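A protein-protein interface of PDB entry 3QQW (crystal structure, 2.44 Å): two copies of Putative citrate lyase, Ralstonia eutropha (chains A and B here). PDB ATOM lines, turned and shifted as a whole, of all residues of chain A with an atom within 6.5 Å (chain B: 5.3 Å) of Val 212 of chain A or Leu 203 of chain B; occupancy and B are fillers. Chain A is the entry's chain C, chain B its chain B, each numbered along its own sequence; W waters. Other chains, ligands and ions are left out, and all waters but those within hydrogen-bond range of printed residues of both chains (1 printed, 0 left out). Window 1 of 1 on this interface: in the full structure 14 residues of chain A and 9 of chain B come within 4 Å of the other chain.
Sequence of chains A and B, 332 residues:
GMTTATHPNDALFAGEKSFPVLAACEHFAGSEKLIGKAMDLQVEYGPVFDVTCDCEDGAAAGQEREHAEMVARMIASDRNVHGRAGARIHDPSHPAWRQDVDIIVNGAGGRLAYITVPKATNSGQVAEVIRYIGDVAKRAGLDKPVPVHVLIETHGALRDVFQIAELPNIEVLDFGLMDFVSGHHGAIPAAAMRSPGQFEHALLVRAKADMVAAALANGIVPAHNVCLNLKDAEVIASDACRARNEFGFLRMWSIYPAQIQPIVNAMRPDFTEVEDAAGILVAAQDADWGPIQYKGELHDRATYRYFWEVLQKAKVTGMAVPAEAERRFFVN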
ATOM      1  N   VAL A 161      27.190  12.963  -2.976  1.00  0.00           N
ATOM      2  CA  VAL A 161      26.044  12.357  -2.287  1.00  0.00           C
ATOM      3  C   VAL A 161      24.678  12.608  -3.009  1.00  0.00           C
ATOM      4  O   VAL A 161      23.885  11.656  -3.122  1.00  0.00           O
ATOM      5  CB  VAL A 161      25.979  12.671  -0.781  1.00  0.00           C
ATOM      6  CG1 VAL A 161      25.548  14.121  -0.483  1.00  0.00           C
ATOM      7  CG2 VAL A 161      25.109  11.641  -0.063  1.00  0.00           C
ATOM      8  N   LEU A 173      21.313   5.009   2.365  1.00  0.00           N
ATOM      9  CA  LEU A 173      22.594   5.706   2.391  1.00  0.00           C
ATOM     10  C   LEU A 173      23.116   5.502   3.793  1.00  0.00           C
ATOM     11  O   LEU A 173      22.447   5.861   4.766  1.00  0.00           O
ATOM     12  CB  LEU A 173      22.539   7.189   2.011  1.00  0.00           C
ATOM     13  CG  LEU A 173      22.121   7.548   0.575  1.00  0.00           C
ATOM     14  CD1 LEU A 173      22.269   9.041   0.346  1.00  0.00           C
ATOM     15  CD2 LEU A 173      22.961   6.775  -0.478  1.00  0.00           C
ATOM     16  N   ALA A 207      28.744  16.501   7.185  1.00  0.00           N
ATOM     17  CA  ALA A 207      28.703  15.245   6.455  1.00  0.00           C
ATOM     18  C   ALA A 207      27.390  14.483   6.726  1.00  0.00           C
ATOM     19  O   ALA A 207      26.683  14.120   5.790  1.00  0.00           O
ATOM     20  CB  ALA A 207      29.898  14.396   6.850  1.00  0.00           C
ATOM     21  N   LYS A 208      27.036  14.298   8.014  1.00  0.00           N
ATOM     22  CA  LYS A 208      25.806  13.605   8.406  1.00  0.00           C
ATOM     23  C   LYS A 208      24.553  14.326   7.862  1.00  0.00           C
ATOM     24  O   LYS A 208      23.679  13.679   7.263  1.00  0.00           O
ATOM     25  CB  LYS A 208      25.718  13.456   9.927  1.00  0.00           C
ATOM     26  CG  LYS A 208      26.672  12.421  10.451  1.00  0.00           C
ATOM     27  CD  LYS A 208      26.481  12.204  11.950  1.00  0.00           C
ATOM     28  CE  LYS A 208      27.385  11.106  12.454  1.00  0.00           C
ATOM     29  NZ  LYS A 208      27.300  10.987  13.930  1.00  0.00           N
ATOM     30  N   ALA A 209      24.478  15.657   8.061  1.00  0.00           N
ATOM     31  CA  ALA A 209      23.331  16.440   7.602  1.00  0.00           C
ATOM     32  C   ALA A 209      23.215  16.398   6.067  1.00  0.00           C
ATOM     33  O   ALA A 209      22.098  16.228   5.576  1.00  0.00           O
ATOM     34  CB  ALA A 209      23.425  17.877   8.112  1.00  0.00           C
ATOM     35  N   ASP A 210      24.356  16.462   5.321  1.00  0.00           N
ATOM     36  CA  ASP A 210      24.322  16.392   3.852  1.00  0.00           C
ATOM     37  C   ASP A 210      23.789  15.067   3.368  1.00  0.00           C
ATOM     38  O   ASP A 210      22.963  15.038   2.455  1.00  0.00           O
ATOM     39  CB  ASP A 210      25.706  16.607   3.237  1.00  0.00           C
ATOM     40  CG  ASP A 210      26.056  18.054   2.994  1.00  0.00           C
ATOM     41  OD1 ASP A 210      25.244  18.928   3.356  1.00  0.00           O
ATOM     42  OD2 ASP A 210      27.148  18.315   2.440  1.00  0.00           O
ATOM     43  N   MET A 211      24.255  13.967   3.979  1.00  0.00           N
ATOM     44  CA  MET A 211      23.844  12.651   3.568  1.00  0.00           C
ATOM     45  C   MET A 211      22.345  12.414   3.851  1.00  0.00           C
ATOM     46  O   MET A 211      21.645  11.868   2.976  1.00  0.00           O
ATOM     47  CB  MET A 211      24.722  11.606   4.236  1.00  0.00           C
ATOM     48  CG  MET A 211      24.602  10.222   3.553  1.00  0.00           C
ATOM     49  SD  MET A 211      24.837   8.722   4.766  1.00  0.00           S
ATOM     50  CE  MET A 211      23.330   8.955   5.786  1.00  0.00           C
ATOM     51  N   VAL A 212      21.854  12.831   5.047  1.00  0.00           N
ATOM     52  CA  VAL A 212      20.444  12.682   5.409  1.00  0.00           C
ATOM     53  C   VAL A 212      19.591  13.526   4.438  1.00  0.00           C
ATOM     54  O   VAL A 212      18.611  13.021   3.894  1.00  0.00           O
ATOM     55  CB  VAL A 212      20.172  13.038   6.886  1.00  0.00           C
ATOM     56  CG1 VAL A 212      18.674  13.099   7.185  1.00  0.00           C
ATOM     57  CG2 VAL A 212      20.851  12.039   7.809  1.00  0.00           C
ATOM     58  N   ALA A 213      20.004  14.776   4.184  1.00  0.00           N
ATOM     59  CA  ALA A 213      19.317  15.667   3.255  1.00  0.00           C
ATOM     60  C   ALA A 213      19.210  15.048   1.849  1.00  0.00           C
ATOM     61  O   ALA A 213      18.143  15.123   1.252  1.00  0.00           O
ATOM     62  CB  ALA A 213      20.035  17.019   3.190  1.00  0.00           C
ATOM     63  N   ALA A 214      20.301  14.412   1.352  1.00  0.00           N
ATOM     64  CA  ALA A 214      20.361  13.775   0.033  1.00  0.00           C
ATOM     65  C   ALA A 214      19.461  12.549  -0.038  1.00  0.00           C
ATOM     66  O   ALA A 214      18.787  12.343  -1.043  1.00  0.00           O
ATOM     67  CB  ALA A 214      21.794  13.390  -0.302  1.00  0.00           C
ATOM     68  N   ALA A 215      19.471  11.736   1.033  1.00  0.00           N
ATOM     69  CA  ALA A 215      18.694  10.517   1.150  1.00  0.00           C
ATOM     70  C   ALA A 215      17.216  10.837   1.172  1.00  0.00           C
ATOM     71  O   ALA A 215      16.467  10.360   0.298  1.00  0.00           O
ATOM     72  CB  ALA A 215      19.098   9.757   2.407  1.00  0.00           C
ATOM     73  N   LEU A 216      16.800  11.714   2.109  1.00  0.00           N
ATOM     74  CA  LEU A 216      15.399  12.094   2.258  1.00  0.00           C
ATOM     75  C   LEU A 216      14.872  12.835   1.032  1.00  0.00           C
ATOM     76  O   LEU A 216      13.718  12.631   0.675  1.00  0.00           O
ATOM     77  CB  LEU A 216      15.155  12.894   3.538  1.00  0.00           C
ATOM     78  CG  LEU A 216      15.449  12.156   4.844  1.00  0.00           C
ATOM     79  CD1 LEU A 216      15.280  13.068   6.000  1.00  0.00           C
ATOM     80  CD2 LEU A 216      14.610  10.891   4.991  1.00  0.00           C
ATOM     81  N   ALA A 217      15.721  13.610   0.344  1.00  0.00           N
ATOM     82  CA  ALA A 217      15.322  14.303  -0.890  1.00  0.00           C
ATOM     83  C   ALA A 217      14.980  13.320  -2.003  1.00  0.00           C
ATOM     84  O   ALA A 217      14.253  13.677  -2.915  1.00  0.00           O
ATOM     85  CB  ALA A 217      16.434  15.226  -1.361  1.00  0.00           C
ATOM     86  N   ILE A 220      15.075   7.917   0.083  1.00  0.00           N
ATOM     87  CA  ILE A 220      16.042   6.925   0.541  1.00  0.00           C
ATOM     88  C   ILE A 220      16.134   7.037   2.049  1.00  0.00           C
ATOM     89  O   ILE A 220      16.068   8.137   2.590  1.00  0.00           O
ATOM     90  CB  ILE A 220      17.424   7.118  -0.167  1.00  0.00           C
ATOM     91  CG1 ILE A 220      17.306   6.809  -1.687  1.00  0.00           C
ATOM     92  CG2 ILE A 220      18.513   6.277   0.458  1.00  0.00           C
ATOM     93  CD1 ILE A 220      18.419   7.361  -2.497  1.00  0.00           C
ATOM     94  N   PRO A 222      18.087   7.241   5.403  1.00  0.00           N
ATOM     95  CA  PRO A 222      19.458   7.520   5.871  1.00  0.00           C
ATOM     96  C   PRO A 222      19.766   6.646   7.100  1.00  0.00           C
ATOM     97  O   PRO A 222      18.979   6.621   8.039  1.00  0.00           O
ATOM     98  CB  PRO A 222      19.427   9.020   6.189  1.00  0.00           C
ATOM     99  CG  PRO A 222      17.932   9.373   6.327  1.00  0.00           C
ATOM    100  CD  PRO A 222      17.108   8.151   6.029  1.00  0.00           C
ATOM    101  N   ALA A 223      20.894   5.898   7.078  1.00  0.00           N
ATOM    102  CA  ALA A 223      21.276   5.032   8.187  1.00  0.00           C
ATOM    103  C   ALA A 223      22.530   5.527   8.886  1.00  0.00           C
ATOM    104  O   ALA A 223      23.475   6.030   8.257  1.00  0.00           O
ATOM    105  CB  ALA A 223      21.457   3.609   7.723  1.00  0.00           C
ATOM    106  N   ALA A 243      20.782  10.649  16.637  1.00  0.00           N
ATOM    107  CA  ALA A 243      20.781  10.457  15.187  1.00  0.00           C
ATOM    108  C   ALA A 243      19.371  10.612  14.650  1.00  0.00           C
ATOM    109  O   ALA A 243      19.183  11.291  13.633  1.00  0.00           O
ATOM    110  CB  ALA A 243      21.342   9.090  14.833  1.00  0.00           C
ATOM    111  N   GLU A 246      18.001  14.672  16.043  1.00  0.00           N
ATOM    112  CA  GLU A 246      18.767  15.880  15.712  1.00  0.00           C
ATOM    113  C   GLU A 246      19.233  15.890  14.253  1.00  0.00           C
ATOM    114  O   GLU A 246      19.489  16.969  13.707  1.00  0.00           O
ATOM    115  CB  GLU A 246      19.996  16.028  16.624  1.00  0.00           C
ATOM    116  CG  GLU A 246      19.695  16.201  18.102  1.00  0.00           C
ATOM    117  CD  GLU A 246      20.930  16.229  18.985  1.00  0.00           C
ATOM    118  OE1 GLU A 246      21.934  16.887  18.611  1.00  0.00           O
ATOM    119  OE2 GLU A 246      20.882  15.603  20.069  1.00  0.00           O
ATOM    120  N   PHE A 247      19.359  14.707  13.626  1.00  0.00           N
ATOM    121  CA  PHE A 247      19.866  14.621  12.267  1.00  0.00           C
ATOM    122  C   PHE A 247      18.880  14.022  11.240  1.00  0.00           C
ATOM    123  O   PHE A 247      19.047  14.292  10.063  1.00  0.00           O
ATOM    124  CB  PHE A 247      21.183  13.829  12.253  1.00  0.00           C
ATOM    125  CG  PHE A 247      22.338  14.610  12.845  1.00  0.00           C
ATOM    126  CD1 PHE A 247      22.558  14.623  14.215  1.00  0.00           C
ATOM    127  CD2 PHE A 247      23.189  15.352  12.031  1.00  0.00           C
ATOM    128  CE1 PHE A 247      23.597  15.375  14.759  1.00  0.00           C
ATOM    129  CE2 PHE A 247      24.242  16.086  12.576  1.00  0.00           C
ATOM    130  CZ  PHE A 247      24.439  16.095  13.933  1.00  0.00           C
ATOM    131  N   GLY A 248      17.875  13.260  11.676  1.00  0.00           N
ATOM    132  CA  GLY A 248      16.897  12.678  10.762  1.00  0.00           C
ATOM    133  C   GLY A 248      17.226  11.294  10.220  1.00  0.00           C
ATOM    134  O   GLY A 248      16.706  10.905   9.167  1.00  0.00           O
ATOM    135  N   PHE A 249      18.093  10.536  10.943  1.00  0.00           N
ATOM    136  CA  PHE A 249      18.417   9.152  10.595  1.00  0.00           C
ATOM    137  C   PHE A 249      17.227   8.293  10.973  1.00  0.00           C
ATOM    138  O   PHE A 249      16.542   8.604  11.951  1.00  0.00           O
ATOM    139  CB  PHE A 249      19.691   8.680  11.299  1.00  0.00           C
ATOM    140  CG  PHE A 249      20.952   9.289  10.740  1.00  0.00           C
ATOM    141  CD1 PHE A 249      21.627   8.684   9.691  1.00  0.00           C
ATOM    142  CD2 PHE A 249      21.491  10.437  11.293  1.00  0.00           C
ATOM    143  CE1 PHE A 249      22.837   9.206   9.216  1.00  0.00           C
ATOM    144  CE2 PHE A 249      22.689  10.971  10.804  1.00  0.00           C
ATOM    145  CZ  PHE A 249      23.355  10.355   9.769  1.00  0.00           C
ATOM    146  N   PHE B 180       8.725  22.506   4.169  1.00  0.00           N
ATOM    147  CA  PHE B 180      10.043  21.894   4.110  1.00  0.00           C
ATOM    148  C   PHE B 180      10.091  20.654   5.012  1.00  0.00           C
ATOM    149  O   PHE B 180      10.504  19.584   4.551  1.00  0.00           O
ATOM    150  CB  PHE B 180      11.148  22.929   4.478  1.00  0.00           C
ATOM    151  CG  PHE B 180      12.540  22.355   4.375  1.00  0.00           C
ATOM    152  CD1 PHE B 180      13.062  21.975   3.141  1.00  0.00           C
ATOM    153  CD2 PHE B 180      13.294  22.106   5.520  1.00  0.00           C
ATOM    154  CE1 PHE B 180      14.319  21.369   3.058  1.00  0.00           C
ATOM    155  CE2 PHE B 180      14.553  21.509   5.432  1.00  0.00           C
ATOM    156  CZ  PHE B 180      15.067  21.171   4.204  1.00  0.00           C
ATOM    157  N   HIS B 184       9.901  15.571   4.687  1.00  0.00           N
ATOM    158  CA  HIS B 184      10.972  14.749   5.241  1.00  0.00           C
ATOM    159  C   HIS B 184      10.537  13.365   5.757  1.00  0.00           C
ATOM    160  O   HIS B 184      11.298  12.749   6.509  1.00  0.00           O
ATOM    161  CB  HIS B 184      11.729  15.519   6.325  1.00  0.00           C
ATOM    162  CG  HIS B 184      12.709  16.491   5.744  1.00  0.00           C
ATOM    163  ND1 HIS B 184      12.305  17.709   5.243  1.00  0.00           N
ATOM    164  CD2 HIS B 184      14.048  16.377   5.578  1.00  0.00           C
ATOM    165  CE1 HIS B 184      13.404  18.300   4.809  1.00  0.00           C
ATOM    166  NE2 HIS B 184      14.478  17.540   4.995  1.00  0.00           N
ATOM    167  N   ILE B 188      12.006  14.615  10.504  1.00  0.00           N
ATOM    168  CA  ILE B 188      12.117  15.844  11.299  1.00  0.00           C
ATOM    169  C   ILE B 188      10.891  15.852  12.223  1.00  0.00           C
ATOM    170  O   ILE B 188       9.759  15.885  11.722  1.00  0.00           O
ATOM    171  CB  ILE B 188      12.255  17.144  10.459  1.00  0.00           C
ATOM    172  CG1 ILE B 188      13.490  17.085   9.550  1.00  0.00           C
ATOM    173  CG2 ILE B 188      12.272  18.382  11.367  1.00  0.00           C
ATOM    174  CD1 ILE B 188      13.635  18.259   8.591  1.00  0.00           C
ATOM    175  N   HIS B 201      17.906  21.985  14.928  1.00  0.00           N
ATOM    176  CA  HIS B 201      17.908  20.713  14.211  1.00  0.00           C
ATOM    177  C   HIS B 201      18.880  20.828  13.028  1.00  0.00           C
ATOM    178  O   HIS B 201      18.791  21.791  12.254  1.00  0.00           O
ATOM    179  CB  HIS B 201      16.487  20.345  13.743  1.00  0.00           C
ATOM    180  CG  HIS B 201      16.387  18.955  13.188  1.00  0.00           C
ATOM    181  ND1 HIS B 201      16.811  18.652  11.895  1.00  0.00           N
ATOM    182  CD2 HIS B 201      15.920  17.826  13.766  1.00  0.00           C
ATOM    183  CE1 HIS B 201      16.572  17.361  11.729  1.00  0.00           C
ATOM    184  NE2 HIS B 201      16.045  16.818  12.829  1.00  0.00           N
ATOM    185  N   ALA B 202      19.823  19.863  12.916  1.00  0.00           N
ATOM    186  CA  ALA B 202      20.869  19.829  11.907  1.00  0.00           C
ATOM    187  C   ALA B 202      20.354  20.066  10.489  1.00  0.00           C
ATOM    188  O   ALA B 202      20.994  20.814   9.747  1.00  0.00           O
ATOM    189  CB  ALA B 202      21.620  18.524  11.975  1.00  0.00           C
ATOM    190  N   LEU B 203      19.183  19.508  10.133  1.00  0.00           N
ATOM    191  CA  LEU B 203      18.624  19.682   8.792  1.00  0.00           C
ATOM    192  C   LEU B 203      18.051  21.070   8.592  1.00  0.00           C
ATOM    193  O   LEU B 203      18.111  21.612   7.482  1.00  0.00           O
ATOM    194  CB  LEU B 203      17.577  18.619   8.462  1.00  0.00           C
ATOM    195  CG  LEU B 203      18.074  17.152   8.421  1.00  0.00           C
ATOM    196  CD1 LEU B 203      16.939  16.227   8.012  1.00  0.00           C
ATOM    197  CD2 LEU B 203      19.272  16.970   7.495  1.00  0.00           C
ATOM    198  N   LEU B 204      17.522  21.661   9.658  1.00  0.00           N
ATOM    199  CA  LEU B 204      16.926  22.999   9.581  1.00  0.00           C
ATOM    200  C   LEU B 204      17.996  24.085   9.621  1.00  0.00           C
ATOM    201  O   LEU B 204      17.892  25.050   8.869  1.00  0.00           O
ATOM    202  CB  LEU B 204      15.895  23.175  10.697  1.00  0.00           C
ATOM    203  CG  LEU B 204      14.740  22.157  10.622  1.00  0.00           C
ATOM    204  CD1 LEU B 204      13.774  22.378  11.719  1.00  0.00           C
ATOM    205  CD2 LEU B 204      14.028  22.234   9.288  1.00  0.00           C
ATOM    206  N   VAL B 205      19.067  23.876  10.423  1.00  0.00           N
ATOM    207  CA  VAL B 205      20.223  24.778  10.472  1.00  0.00           C
ATOM    208  C   VAL B 205      20.847  24.808   9.059  1.00  0.00           C
ATOM    209  O   VAL B 205      21.092  25.881   8.512  1.00  0.00           O
ATOM    210  CB  VAL B 205      21.266  24.377  11.548  1.00  0.00           C
ATOM    211  CG1 VAL B 205      22.493  25.258  11.459  1.00  0.00           C
ATOM    212  CG2 VAL B 205      20.671  24.454  12.945  1.00  0.00           C
ATOM    213  N   ARG B 206      21.048  23.619   8.478  1.00  0.00           N
ATOM    214  CA  ARG B 206      21.628  23.406   7.166  1.00  0.00           C
ATOM    215  C   ARG B 206      20.815  24.110   6.098  1.00  0.00           C
ATOM    216  O   ARG B 206      21.379  24.855   5.299  1.00  0.00           O
ATOM    217  CB  ARG B 206      21.730  21.900   6.878  1.00  0.00           C
ATOM    218  CG  ARG B 206      22.258  21.561   5.511  1.00  0.00           C
ATOM    219  CD  ARG B 206      22.147  20.079   5.225  1.00  0.00           C
ATOM    220  NE  ARG B 206      22.628  19.791   3.879  1.00  0.00           N
ATOM    221  CZ  ARG B 206      21.890  19.925   2.791  1.00  0.00           C
ATOM    222  NH1 ARG B 206      20.618  20.280   2.887  1.00  0.00           N
ATOM    223  NH2 ARG B 206      22.405  19.668   1.600  1.00  0.00           N
ATOM    224  N   ALA B 207      19.495  23.891   6.096  1.00  0.00           N
ATOM    225  CA  ALA B 207      18.565  24.489   5.143  1.00  0.00           C
ATOM    226  C   ALA B 207      18.557  26.009   5.263  1.00  0.00           C
ATOM    227  O   ALA B 207      18.774  26.687   4.265  1.00  0.00           O
ATOM    228  CB  ALA B 207      17.183  23.939   5.369  1.00  0.00           C
ATOM    229  N   LYS B 208      18.372  26.545   6.483  1.00  0.00           N
ATOM    230  CA  LYS B 208      18.331  27.990   6.730  1.00  0.00           C
ATOM    231  C   LYS B 208      19.643  28.652   6.317  1.00  0.00           C
ATOM    232  O   LYS B 208      19.605  29.629   5.554  1.00  0.00           O
ATOM    233  CB  LYS B 208      17.992  28.295   8.195  1.00  0.00           C
ATOM    234  CG  LYS B 208      16.525  28.056   8.507  1.00  0.00           C
ATOM    235  CD  LYS B 208      16.156  28.432   9.917  1.00  0.00           C
ATOM    236  CE  LYS B 208      14.663  28.263  10.145  1.00  0.00           C
ATOM    237  NZ  LYS B 208      14.268  28.684  11.521  1.00  0.00           N
HETATM  238  O   HOH W   1      15.309  14.449  13.102  1.00  0.00           O
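Water W1 lies within hydrogen-bond range of NE2 of His 201 of chain B and N of Gly 248 of chain A.
Val 212 of chain A touches one residue of chain B. Printed residues of chain B within 4 Å of Ala 213 of chain A: Arg 206. Printed residues of chain B within 4 Å of Glu 246 of chain A: His 201 (3.5 Å) and Ala 202 (3.0 Å). Of the printed residues of chain A, His 184 of chain B touches Leu 216 (3.6 Å). Of the printed residues of chain A, His 201 of chain B touches Glu 246 (3.5 Å). Of chain A, only Ala 209 (3.5 Å), Val 212 (3.7 Å) and Phe 247 (3.4 Å) come within 4 Å of Leu 203 of chain B. Printed residues of chain A within 4 Å of Arg 206 of chain B: Ala 209 (3.8 Å), Asp 210 (2.8 Å) and Ala 213 (3.3 Å). The nearest residue of chain A that does not touch Leu 203 of chain B is Ala 213 of chain A (4.04 Å). The nearest printed residue of chain B that does not touch Ala 209 of chain A is Ala 202 of chain B (4.1 Å).
Leu 203 of chain B touches Ala 209 of chain A. CB of Ala 209 of chain A touches CD of Arg 206 of chain B (3.8 Å). CG1 of Val 212 of chain A touches CD1 of Leu 203 of chain B (3.7 Å). Ala 213 of chain A touches Arg 206 of chain B (CB to NH1, 3.3 Å). CD1 of Leu 216 of chain A touches CD2 of His 184 of chain B, 3.6 Å away. O of Glu 246 of chain A touches CE1 of His 201 of chain B (3.5 Å). Phe 247 of chain A touches Ala 202 of chain B (CD2 to CB, 3.5 Å). Phe 247 of chain A touches Leu 203 of chain B.
Of the 11 printed residues of chain B, 5 touch a printed residue of chain A. Hydrophobic or aromatic side chains of chain B that line the printed part of chain A: His 184, His 201, Ala 202 and Leu 203. Along chain B the printed residues that touch a printed residue of chain A span positions 184 to 206. Of the 21 printed residues of chain A, 7 touch a printed residue of chain B. Hydrophobic or aromatic side chains of chain A within 4 Å of the printed part of chain B: Ala 209, Val 212, Ala 213, Leu 216 and Phe 247. Among the printed residues, Asp or Glu carboxylates within 4 Å of a Lys or Arg side-chain nitrogen of the other chain: Asp 210 of chain A with Arg 206 of chain B (2.8 Å).
Positions printed for both chains: 207 and 208.
ND1 of His 201 of chain B lies within hydrogen-bond range of N of Leu 203 of chain B (3.1 Å). The backbone carbonyl oxygen (O) of Phe 180 of chain B sits at hydrogen-bond distance from a ring nitrogen (ND1) of His 184 of chain B, 2.7 Å away.
N of Ala 202 of chain B lies within hydrogen-bond range of O of Glu 246 of chain A, 3.0 Å away. NE of Arg 206 of chain B lies within salt-bridge range of OD1 of Asp 210 of chain A (2.8 Å).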
